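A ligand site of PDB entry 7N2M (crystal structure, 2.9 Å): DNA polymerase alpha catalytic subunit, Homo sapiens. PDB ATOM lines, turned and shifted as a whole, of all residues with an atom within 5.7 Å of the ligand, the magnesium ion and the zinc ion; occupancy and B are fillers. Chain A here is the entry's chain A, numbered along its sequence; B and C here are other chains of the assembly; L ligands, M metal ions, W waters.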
ATOM      1  N   ASP A 525       6.840 -25.642 -22.137  1.00  0.00           N
ATOM      2  CA  ASP A 525       6.661 -24.193 -22.184  1.00  0.00           C
ATOM      3  C   ASP A 525       5.250 -23.805 -21.724  1.00  0.00           C
ATOM      4  O   ASP A 525       4.275 -24.454 -22.106  1.00  0.00           O
ATOM      5  CB  ASP A 525       6.897 -23.658 -23.608  1.00  0.00           C
ATOM      6  CG  ASP A 525       6.819 -22.120 -23.699  1.00  0.00           C
ATOM      7  OD1 ASP A 525       7.793 -21.424 -23.342  1.00  0.00           O
ATOM      8  OD2 ASP A 525       5.756 -21.611 -24.119  1.00  0.00           O
ATOM      9  N   PHE A 526       5.141 -22.762 -20.919  1.00  0.00           N
ATOM     10  CA  PHE A 526       3.818 -22.300 -20.498  1.00  0.00           C
ATOM     11  C   PHE A 526       3.063 -21.617 -21.651  1.00  0.00           C
ATOM     12  O   PHE A 526       3.643 -20.913 -22.492  1.00  0.00           O
ATOM     13  CB  PHE A 526       3.925 -21.310 -19.356  1.00  0.00           C
ATOM     14  CG  PHE A 526       4.256 -21.933 -18.047  1.00  0.00           C
ATOM     15  CD1 PHE A 526       5.549 -21.912 -17.551  1.00  0.00           C
ATOM     16  CD2 PHE A 526       3.257 -22.520 -17.284  1.00  0.00           C
ATOM     17  CE1 PHE A 526       5.845 -22.473 -16.312  1.00  0.00           C
ATOM     18  CE2 PHE A 526       3.546 -23.074 -16.044  1.00  0.00           C
ATOM     19  CZ  PHE A 526       4.843 -23.047 -15.559  1.00  0.00           C
ATOM     20  N   ASN A 527       1.757 -21.847 -21.678  1.00  0.00           N
ATOM     21  CA  ASN A 527       0.863 -21.269 -22.673  1.00  0.00           C
ATOM     22  C   ASN A 527       0.528 -19.837 -22.289  1.00  0.00           C
ATOM     23  O   ASN A 527      -0.006 -19.598 -21.195  1.00  0.00           O
ATOM     24  CB  ASN A 527      -0.427 -22.102 -22.775  1.00  0.00           C
ATOM     25  CG  ASN A 527      -0.225 -23.383 -23.526  1.00  0.00           C
ATOM     26  OD1 ASN A 527       0.314 -23.388 -24.635  1.00  0.00           O
ATOM     27  ND2 ASN A 527      -0.664 -24.491 -22.944  1.00  0.00           N
ATOM     28  N   SER A 528       0.836 -18.887 -23.174  1.00  0.00           N
ATOM     29  CA  SER A 528       0.554 -17.478 -22.934  1.00  0.00           C
ATOM     30  C   SER A 528       0.841 -17.026 -21.500  1.00  0.00           C
ATOM     31  O   SER A 528      -0.001 -16.414 -20.838  1.00  0.00           O
ATOM     32  CB  SER A 528      -0.911 -17.187 -23.288  1.00  0.00           C
ATOM     33  OG  SER A 528      -1.094 -17.166 -24.694  1.00  0.00           O
ATOM     34  N   LEU A 529       2.060 -17.307 -21.048  1.00  0.00           N
ATOM     35  CA  LEU A 529       2.452 -16.996 -19.696  1.00  0.00           C
ATOM     36  C   LEU A 529       2.065 -15.633 -19.148  1.00  0.00           C
ATOM     37  O   LEU A 529       1.207 -15.538 -18.282  1.00  0.00           O
ATOM     38  CB  LEU A 529       3.963 -17.208 -19.526  1.00  0.00           C
ATOM     39  CG  LEU A 529       4.424 -16.984 -18.089  1.00  0.00           C
ATOM     40  CD1 LEU A 529       3.753 -17.996 -17.183  1.00  0.00           C
ATOM     41  CD2 LEU A 529       5.917 -17.097 -17.998  1.00  0.00           C
ATOM     42  N   TYR A 530       2.689 -14.560 -19.635  1.00  0.00           N
ATOM     43  CA  TYR A 530       2.362 -13.250 -19.096  1.00  0.00           C
ATOM     44  C   TYR A 530       0.865 -12.935 -19.155  1.00  0.00           C
ATOM     45  O   TYR A 530       0.281 -12.446 -18.179  1.00  0.00           O
ATOM     46  CB  TYR A 530       3.203 -12.186 -19.799  1.00  0.00           C
ATOM     47  CG  TYR A 530       4.637 -12.112 -19.311  1.00  0.00           C
ATOM     48  CD1 TYR A 530       5.323 -13.263 -18.909  1.00  0.00           C
ATOM     49  CD2 TYR A 530       5.314 -10.907 -19.309  1.00  0.00           C
ATOM     50  CE1 TYR A 530       6.661 -13.206 -18.520  1.00  0.00           C
ATOM     51  CE2 TYR A 530       6.651 -10.835 -18.921  1.00  0.00           C
ATOM     52  CZ  TYR A 530       7.319 -11.990 -18.535  1.00  0.00           C
ATOM     53  OH  TYR A 530       8.658 -11.922 -18.199  1.00  0.00           O
ATOM     54  N   PRO A 531       0.204 -13.170 -20.306  1.00  0.00           N
ATOM     55  CA  PRO A 531      -1.229 -12.868 -20.318  1.00  0.00           C
ATOM     56  C   PRO A 531      -1.967 -13.679 -19.252  1.00  0.00           C
ATOM     57  O   PRO A 531      -2.878 -13.158 -18.594  1.00  0.00           O
ATOM     58  CB  PRO A 531      -1.635 -13.214 -21.735  1.00  0.00           C
ATOM     59  CG  PRO A 531      -0.432 -12.713 -22.517  1.00  0.00           C
ATOM     60  CD  PRO A 531       0.717 -13.280 -21.698  1.00  0.00           C
ATOM     61  N   ARG A 587      -6.790 -16.358 -30.068  1.00  0.00           N
ATOM     62  CA  ARG A 587      -5.626 -17.102 -30.484  1.00  0.00           C
ATOM     63  C   ARG A 587      -5.859 -18.608 -30.405  1.00  0.00           C
ATOM     64  O   ARG A 587      -5.556 -19.322 -31.363  1.00  0.00           O
ATOM     65  CB  ARG A 587      -4.436 -16.710 -29.640  1.00  0.00           C
ATOM     66  CG  ARG A 587      -3.130 -17.214 -30.197  1.00  0.00           C
ATOM     67  CD  ARG A 587      -2.040 -17.098 -29.166  1.00  0.00           C
ATOM     68  NE  ARG A 587      -0.885 -17.871 -29.567  1.00  0.00           N
ATOM     69  CZ  ARG A 587       0.100 -18.186 -28.734  1.00  0.00           C
ATOM     70  NH1 ARG A 587       0.056 -17.774 -27.476  1.00  0.00           N
ATOM     71  NH2 ARG A 587       1.122 -18.906 -29.160  1.00  0.00           N
ATOM     72  N   LYS A 591      -5.679 -21.600 -33.224  1.00  0.00           N
ATOM     73  CA  LYS A 591      -4.789 -22.737 -33.089  1.00  0.00           C
ATOM     74  C   LYS A 591      -5.622 -23.978 -33.288  1.00  0.00           C
ATOM     75  O   LYS A 591      -5.161 -24.954 -33.863  1.00  0.00           O
ATOM     76  CB  LYS A 591      -4.094 -22.723 -31.726  1.00  0.00           C
ATOM     77  CG  LYS A 591      -3.319 -21.437 -31.456  1.00  0.00           C
ATOM     78  CD  LYS A 591      -2.213 -21.601 -30.452  1.00  0.00           C
ATOM     79  CE  LYS A 591      -1.070 -22.384 -31.054  1.00  0.00           C
ATOM     80  NZ  LYS A 591       0.021 -22.544 -30.078  1.00  0.00           N
ATOM     81  N   GLN A 611      -1.979 -16.553 -35.830  1.00  0.00           N
ATOM     82  CA  GLN A 611      -1.852 -16.993 -34.450  1.00  0.00           C
ATOM     83  C   GLN A 611      -0.744 -16.273 -33.683  1.00  0.00           C
ATOM     84  O   GLN A 611      -0.916 -15.943 -32.520  1.00  0.00           O
ATOM     85  CB  GLN A 611      -1.635 -18.499 -34.437  1.00  0.00           C
ATOM     86  CG  GLN A 611      -1.379 -19.061 -33.096  1.00  0.00           C
ATOM     87  CD  GLN A 611       0.084 -19.190 -32.830  1.00  0.00           C
ATOM     88  OE1 GLN A 611       0.514 -19.271 -31.684  1.00  0.00           O
ATOM     89  NE2 GLN A 611       0.876 -19.236 -33.902  1.00  0.00           N
ATOM     90  N   LYS A 615      -0.664 -13.420 -30.643  1.00  0.00           N
ATOM     91  CA  LYS A 615       0.223 -13.623 -29.500  1.00  0.00           C
ATOM     92  C   LYS A 615       0.916 -12.294 -29.225  1.00  0.00           C
ATOM     93  O   LYS A 615       0.939 -11.817 -28.092  1.00  0.00           O
ATOM     94  CB  LYS A 615       1.256 -14.691 -29.840  1.00  0.00           C
ATOM     95  CG  LYS A 615       2.218 -15.014 -28.743  1.00  0.00           C
ATOM     96  CD  LYS A 615       3.296 -15.906 -29.309  1.00  0.00           C
ATOM     97  CE  LYS A 615       4.256 -16.418 -28.264  1.00  0.00           C
ATOM     98  NZ  LYS A 615       5.301 -17.223 -28.945  1.00  0.00           N
ATOM     99  N   LEU A 616       1.454 -11.704 -30.293  1.00  0.00           N
ATOM    100  CA  LEU A 616       2.133 -10.421 -30.206  1.00  0.00           C
ATOM    101  C   LEU A 616       1.236  -9.329 -29.632  1.00  0.00           C
ATOM    102  O   LEU A 616       1.670  -8.508 -28.829  1.00  0.00           O
ATOM    103  CB  LEU A 616       2.612  -9.998 -31.583  1.00  0.00           C
ATOM    104  CG  LEU A 616       4.060 -10.427 -31.810  1.00  0.00           C
ATOM    105  CD1 LEU A 616       4.348 -10.668 -33.289  1.00  0.00           C
ATOM    106  CD2 LEU A 616       4.961  -9.343 -31.187  1.00  0.00           C
ATOM    107  N   ASN A 619       1.059  -9.837 -25.890  1.00  0.00           N
ATOM    108  CA  ASN A 619       2.289  -9.450 -25.210  1.00  0.00           C
ATOM    109  C   ASN A 619       2.525  -7.947 -25.248  1.00  0.00           C
ATOM    110  O   ASN A 619       2.984  -7.351 -24.273  1.00  0.00           O
ATOM    111  CB  ASN A 619       3.463 -10.215 -25.801  1.00  0.00           C
ATOM    112  CG  ASN A 619       3.418 -11.690 -25.450  1.00  0.00           C
ATOM    113  OD1 ASN A 619       4.042 -12.518 -26.101  1.00  0.00           O
ATOM    114  ND2 ASN A 619       2.656 -12.028 -24.407  1.00  0.00           N
ATOM    115  N   TYR A 622       0.995  -6.301 -22.474  1.00  0.00           N
ATOM    116  CA  TYR A 622       1.800  -6.353 -21.244  1.00  0.00           C
ATOM    117  C   TYR A 622       2.875  -5.286 -21.374  1.00  0.00           C
ATOM    118  O   TYR A 622       3.044  -4.442 -20.490  1.00  0.00           O
ATOM    119  CB  TYR A 622       2.460  -7.735 -21.091  1.00  0.00           C
ATOM    120  CG  TYR A 622       3.871  -7.684 -20.522  1.00  0.00           C
ATOM    121  CD1 TYR A 622       4.102  -7.339 -19.198  1.00  0.00           C
ATOM    122  CD2 TYR A 622       4.985  -7.892 -21.354  1.00  0.00           C
ATOM    123  CE1 TYR A 622       5.414  -7.175 -18.711  1.00  0.00           C
ATOM    124  CE2 TYR A 622       6.284  -7.739 -20.894  1.00  0.00           C
ATOM    125  CZ  TYR A 622       6.498  -7.366 -19.568  1.00  0.00           C
ATOM    126  OH  TYR A 622       7.792  -7.142 -19.114  1.00  0.00           O
ATOM    127  N   ASP A 667      14.191 -20.739 -20.253  1.00  0.00           N
ATOM    128  CA  ASP A 667      14.098 -19.331 -20.678  1.00  0.00           C
ATOM    129  C   ASP A 667      12.720 -18.675 -20.440  1.00  0.00           C
ATOM    130  O   ASP A 667      11.793 -18.877 -21.211  1.00  0.00           O
ATOM    131  CB  ASP A 667      14.467 -19.224 -22.161  1.00  0.00           C
ATOM    132  CG  ASP A 667      14.662 -17.776 -22.618  1.00  0.00           C
ATOM    133  OD1 ASP A 667      14.153 -16.853 -21.953  1.00  0.00           O
ATOM    134  OD2 ASP A 667      15.316 -17.588 -23.661  1.00  0.00           O
ATOM    135  N   THR A 668      12.619 -17.872 -19.384  1.00  0.00           N
ATOM    136  CA  THR A 668      11.397 -17.157 -19.004  1.00  0.00           C
ATOM    137  C   THR A 668      10.198 -18.036 -18.648  1.00  0.00           C
ATOM    138  O   THR A 668       9.676 -17.952 -17.541  1.00  0.00           O
ATOM    139  CB  THR A 668      10.934 -16.171 -20.113  1.00  0.00           C
ATOM    140  OG1 THR A 668      12.055 -15.367 -20.536  1.00  0.00           O
ATOM    141  CG2 THR A 668       9.821 -15.240 -19.564  1.00  0.00           C
ATOM    142  N   ASP A 669       9.755 -18.877 -19.581  1.00  0.00           N
ATOM    143  CA  ASP A 669       8.591 -19.729 -19.349  1.00  0.00           C
ATOM    144  C   ASP A 669       8.810 -21.151 -19.851  1.00  0.00           C
ATOM    145  O   ASP A 669       7.844 -21.862 -20.147  1.00  0.00           O
ATOM    146  CB  ASP A 669       7.341 -19.158 -20.042  1.00  0.00           C
ATOM    147  CG  ASP A 669       7.374 -19.325 -21.592  1.00  0.00           C
ATOM    148  OD1 ASP A 669       6.274 -19.538 -22.176  1.00  0.00           O
ATOM    149  OD2 ASP A 669       8.452 -19.227 -22.230  1.00  0.00           O
ATOM    150  N   SER A 670      10.064 -21.571 -19.971  1.00  0.00           N
ATOM    151  CA  SER A 670      10.336 -22.923 -20.452  1.00  0.00           C
ATOM    152  C   SER A 670      11.318 -23.683 -19.583  1.00  0.00           C
ATOM    153  O   SER A 670      12.024 -23.103 -18.768  1.00  0.00           O
ATOM    154  CB  SER A 670      10.842 -22.895 -21.897  1.00  0.00           C
ATOM    155  OG  SER A 670      11.997 -22.081 -22.061  1.00  0.00           O
ATOM    156  N   ASP A 706       6.274 -28.435 -25.460  1.00  0.00           N
ATOM    157  CA  ASP A 706       6.527 -27.645 -26.667  1.00  0.00           C
ATOM    158  C   ASP A 706       7.277 -28.462 -27.720  1.00  0.00           C
ATOM    159  O   ASP A 706       7.159 -28.205 -28.928  1.00  0.00           O
ATOM    160  CB  ASP A 706       7.306 -26.381 -26.323  1.00  0.00           C
ATOM    161  CG  ASP A 706       7.091 -25.268 -27.339  1.00  0.00           C
ATOM    162  OD1 ASP A 706       5.977 -24.710 -27.391  1.00  0.00           O
ATOM    163  OD2 ASP A 706       8.043 -24.962 -28.093  1.00  0.00           O
ATOM    164  P    DG B   4       5.540   0.575 -30.927  1.00  0.00           P
ATOM    165  OP1  DG B   4       5.983  -0.722 -31.496  1.00  0.00           O
ATOM    166  OP2  DG B   4       4.234   1.159 -31.339  1.00  0.00           O
ATOM    167  O5'  DG B   4       5.492   0.481 -29.346  1.00  0.00           O
ATOM    168  C5'  DG B   4       6.576  -0.052 -28.638  1.00  0.00           C
ATOM    169  C4'  DG B   4       6.112  -0.599 -27.314  1.00  0.00           C
ATOM    170  O4'  DG B   4       5.164  -1.660 -27.556  1.00  0.00           O
ATOM    171  C3'  DG B   4       7.216  -1.243 -26.517  1.00  0.00           C
ATOM    172  O3'  DG B   4       7.719  -0.339 -25.563  1.00  0.00           O
ATOM    173  C2'  DG B   4       6.504  -2.326 -25.738  1.00  0.00           C
ATOM    174  C1'  DG B   4       5.361  -2.733 -26.633  1.00  0.00           C
ATOM    175  N9   DG B   4       5.761  -3.875 -27.435  1.00  0.00           N
ATOM    176  C8   DG B   4       5.903  -3.890 -28.800  1.00  0.00           C
ATOM    177  N7   DG B   4       6.300  -5.045 -29.259  1.00  0.00           N
ATOM    178  C5   DG B   4       6.429  -5.835 -28.132  1.00  0.00           C
ATOM    179  C6   DG B   4       6.832  -7.196 -28.013  1.00  0.00           C
ATOM    180  O6   DG B   4       7.144  -7.983 -28.914  1.00  0.00           O
ATOM    181  N1   DG B   4       6.841  -7.607 -26.691  1.00  0.00           N
ATOM    182  C2   DG B   4       6.505  -6.828 -25.618  1.00  0.00           C
ATOM    183  N2   DG B   4       6.589  -7.394 -24.412  1.00  0.00           N
ATOM    184  N3   DG B   4       6.112  -5.564 -25.719  1.00  0.00           N
ATOM    185  C4   DG B   4       6.097  -5.135 -27.000  1.00  0.00           C
ATOM    186  P    DT B   5       9.225  -0.497 -25.099  1.00  0.00           P
ATOM    187  OP1  DT B   5       9.641   0.737 -24.366  1.00  0.00           O
ATOM    188  OP2  DT B   5       9.944  -0.932 -26.319  1.00  0.00           O
ATOM    189  O5'  DT B   5       9.172  -1.724 -24.100  1.00  0.00           O
ATOM    190  C5'  DT B   5       8.449  -1.624 -22.885  1.00  0.00           C
ATOM    191  C4'  DT B   5       8.749  -2.828 -22.014  1.00  0.00           C
ATOM    192  O4'  DT B   5       8.191  -3.995 -22.658  1.00  0.00           O
ATOM    193  C3'  DT B   5      10.234  -3.124 -21.881  1.00  0.00           C
ATOM    194  O3'  DT B   5      10.720  -2.615 -20.635  1.00  0.00           O
ATOM    195  C2'  DT B   5      10.269  -4.630 -21.721  1.00  0.00           C
ATOM    196  C1'  DT B   5       9.017  -5.129 -22.426  1.00  0.00           C
ATOM    197  N1   DT B   5       9.304  -5.745 -23.721  1.00  0.00           N
ATOM    198  C2   DT B   5       9.539  -7.090 -23.749  1.00  0.00           C
ATOM    199  O2   DT B   5       9.501  -7.789 -22.748  1.00  0.00           O
ATOM    200  N3   DT B   5       9.848  -7.586 -24.990  1.00  0.00           N
ATOM    201  C4   DT B   5       9.930  -6.871 -26.169  1.00  0.00           C
ATOM    202  O4   DT B   5      10.223  -7.445 -27.222  1.00  0.00           O
ATOM    203  C5   DT B   5       9.645  -5.474 -26.062  1.00  0.00           C
ATOM    204  C7   DT B   5       9.707  -4.622 -27.292  1.00  0.00           C
ATOM    205  C6   DT B   5       9.341  -4.980 -24.863  1.00  0.00           C
ATOM    206  P     C C  11      12.764 -17.812 -28.269  1.00  0.00           P
ATOM    207  OP1   C C  11      12.620 -19.285 -28.060  1.00  0.00           O
ATOM    208  OP2   C C  11      12.256 -17.184 -29.526  1.00  0.00           O
ATOM    209  O5'   C C  11      12.146 -16.997 -27.030  1.00  0.00           O
ATOM    210  C5'   C C  11      12.283 -17.521 -25.716  1.00  0.00           C
ATOM    211  C4'   C C  11      12.093 -16.455 -24.667  1.00  0.00           C
ATOM    212  O4'   C C  11      12.656 -15.204 -25.097  1.00  0.00           O
ATOM    213  C3'   C C  11      10.632 -16.123 -24.396  1.00  0.00           C
ATOM    214  C2'   C C  11      10.684 -14.687 -23.887  1.00  0.00           C
ATOM    215  C1'   C C  11      11.913 -14.117 -24.548  1.00  0.00           C
ATOM    216  N1    C C  11      11.605 -13.173 -25.628  1.00  0.00           N
ATOM    217  C2    C C  11      11.151 -11.912 -25.291  1.00  0.00           C
ATOM    218  O2    C C  11      11.013 -11.640 -24.088  1.00  0.00           O
ATOM    219  N3    C C  11      10.868 -11.015 -26.278  1.00  0.00           N
ATOM    220  C4    C C  11      11.014 -11.371 -27.557  1.00  0.00           C
ATOM    221  N4    C C  11      10.721 -10.478 -28.500  1.00  0.00           N
ATOM    222  C5    C C  11      11.477 -12.663 -27.924  1.00  0.00           C
ATOM    223  C6    C C  11      11.758 -13.531 -26.939  1.00  0.00           C
HETATM  224  N1  LIG L   1       7.236 -12.158 -24.273  1.00  0.00           N
HETATM  225  C1  LIG L   1       7.077 -10.810 -24.593  1.00  0.00           C
HETATM  226  N2  LIG L   1       7.193 -10.385 -25.874  1.00  0.00           N
HETATM  227  C2  LIG L   1       7.472 -11.255 -26.872  1.00  0.00           C
HETATM  228  C3  LIG L   1       7.649 -12.654 -26.582  1.00  0.00           C
HETATM  229  C4  LIG L   1       7.514 -13.072 -25.287  1.00  0.00           C
HETATM  230  O1  LIG L   1       6.828  -9.992 -23.721  1.00  0.00           O
HETATM  231  N3  LIG L   1       7.592 -10.810 -28.166  1.00  0.00           N
HETATM  232  C5  LIG L   1       7.096 -12.616 -22.859  1.00  0.00           C
HETATM  233  C6  LIG L   1       5.630 -12.764 -22.537  1.00  0.00           C
HETATM  234  C7  LIG L   1       5.379 -14.241 -22.766  1.00  0.00           C
HETATM  235  C8  LIG L   1       6.675 -14.861 -22.193  1.00  0.00           C
HETATM  236  O2  LIG L   1       7.702 -13.917 -22.639  1.00  0.00           O
HETATM  237  O3  LIG L   1       4.238 -14.654 -22.008  1.00  0.00           O
HETATM  238  C9  LIG L   1       6.990 -16.264 -22.803  1.00  0.00           C
HETATM  239  O4  LIG L   1       7.374 -16.117 -24.160  1.00  0.00           O
HETATM  240  P1  LIG L   1       6.631 -17.163 -25.144  1.00  0.00           P
HETATM  241  O5  LIG L   1       6.621 -18.530 -24.565  1.00  0.00           O
HETATM  242  O6  LIG L   1       7.398 -17.178 -26.575  1.00  0.00           O
HETATM  243  O7  LIG L   1       5.152 -16.532 -25.355  1.00  0.00           O
HETATM  244  P2  LIG L   1       3.933 -17.205 -24.561  1.00  0.00           P
HETATM  245  O8  LIG L   1       4.399 -18.330 -23.500  1.00  0.00           O
HETATM  246  O9  LIG L   1       3.184 -16.181 -23.840  1.00  0.00           O
HETATM  247  O10 LIG L   1       3.039 -17.797 -25.764  1.00  0.00           O
HETATM  248  P3  LIG L   1       3.210 -19.333 -26.068  1.00  0.00           P
HETATM  249  O11 LIG L   1       1.883 -20.080 -25.550  1.00  0.00           O
HETATM  250  O12 LIG L   1       3.384 -19.495 -27.518  1.00  0.00           O
HETATM  251  O13 LIG L   1       4.489 -19.954 -25.325  1.00  0.00           O
HETATM  252 MG    MG M   1       5.048 -20.088 -23.419  1.00  0.00          MG
HETATM  253 ZN    ZN M   2       8.656 -19.748 -24.239  1.00  0.00          ZN
HETATM  254  O   HOH W   1       8.110 -13.132 -29.710  1.00  0.00           O
HETATM  255  O   HOH W   2       1.126 -14.294 -25.222  1.00  0.00           O
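O6 of DG 4 of chain B lies within hydrogen-bond range of a nitrogen (N3) of the ligand (3.0 Å).
The backbone NH (N) of Tyr 530 lies within hydrogen-bond range of an oxygen (O3) of the ligand (2.8 Å).
The guanidinium group (NH2) of Arg 587 lies within salt-bridge range of an oxygen (O12) of the ligand (2.9 Å).
N of Ser 528 is in hydrogen-bond range of O11 of the ligand (2.9 Å).
NZ of Lys 615 is in salt-bridge range of O6 of the ligand (3.2 Å).
A nitrogen (N3) of the ligand sits at hydrogen-bond distance from N4 of C 11 of chain C (3.2 Å).
The backbone NH (N) of Leu 529 is in hydrogen-bond range of an oxygen (O9) of the ligand, 3.2 Å away.
NH1 of Arg 587 lies within hydrogen-bond range of OG of Ser 528 (3.1 Å).
The guanidinium group (NH2) of Arg 587 is in hydrogen-bond range of the side-chain amide oxygen (OE1) of Gln 611, at 2.6 Å.
The side-chain hydroxyl of Thr 668 is in hydrogen-bond range of the side-chain carboxylate of Asp 667 (2.9 Å).
Of the 22 residues printed, 3 come within 4 Å of the magnesium ion.
OD2 of Asp 525 binds the magnesium ion (1.8 Å).
The magnesium ion is bound by OD1 of Asp 669.
O of Phe 526 binds the magnesium ion (1.9 Å).
The magnesium ion is bound by O8 of the ligand.
O13 of the ligand is bound to the magnesium ion, 2.0 Å away.
The magnesium ion is bound by O5 of the ligand, at 2.5 Å.
The magnesium ion has six donor atoms within binding distance.
Within 4 Å of the zinc ion: Asp 525 and Asp 669.
Water W2 bridges the side-chain amide nitrogen (ND2) of Asn 619 (2.9 Å) and an oxygen (O9) of the ligand (3.1 Å).
CA of Asn 527 touches O11 of the ligand, at 3.3 Å.
Pro 531 touches the ligand.
Asn 619 touches the ligand.
CE2 of Tyr 622 touches O1 of the ligand, 3.7 Å away.
Thr 668 touches the ligand.
DT 5 of chain B touches the ligand.
Hydrophobic or aromatic side chains within 4 Å of the ligand: Leu 529, Tyr 530, Pro 531 and Tyr 622.
16 residues have an atom within 4 Å of the ligand: Asp 525, Phe 526, Asn 527, Ser 528, Leu 529, Tyr 530, Pro 531, Arg 587, Lys 615, Asn 619, Tyr 622, Thr 668, Asp 669, DG 4 of chain B, DT 5 of chain B and C 11 of chain C.
Along chain A the residues within 4 Å of the ligand span positions 525 to 669.
The nearest printed residue that does not touch the ligand is Leu 616 (4.3 Å).
The zinc ion is bound by the side-chain carboxylate of Asp 669, the side-chain carboxylate of Asp 525 and an oxygen (O5) of the ligand.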
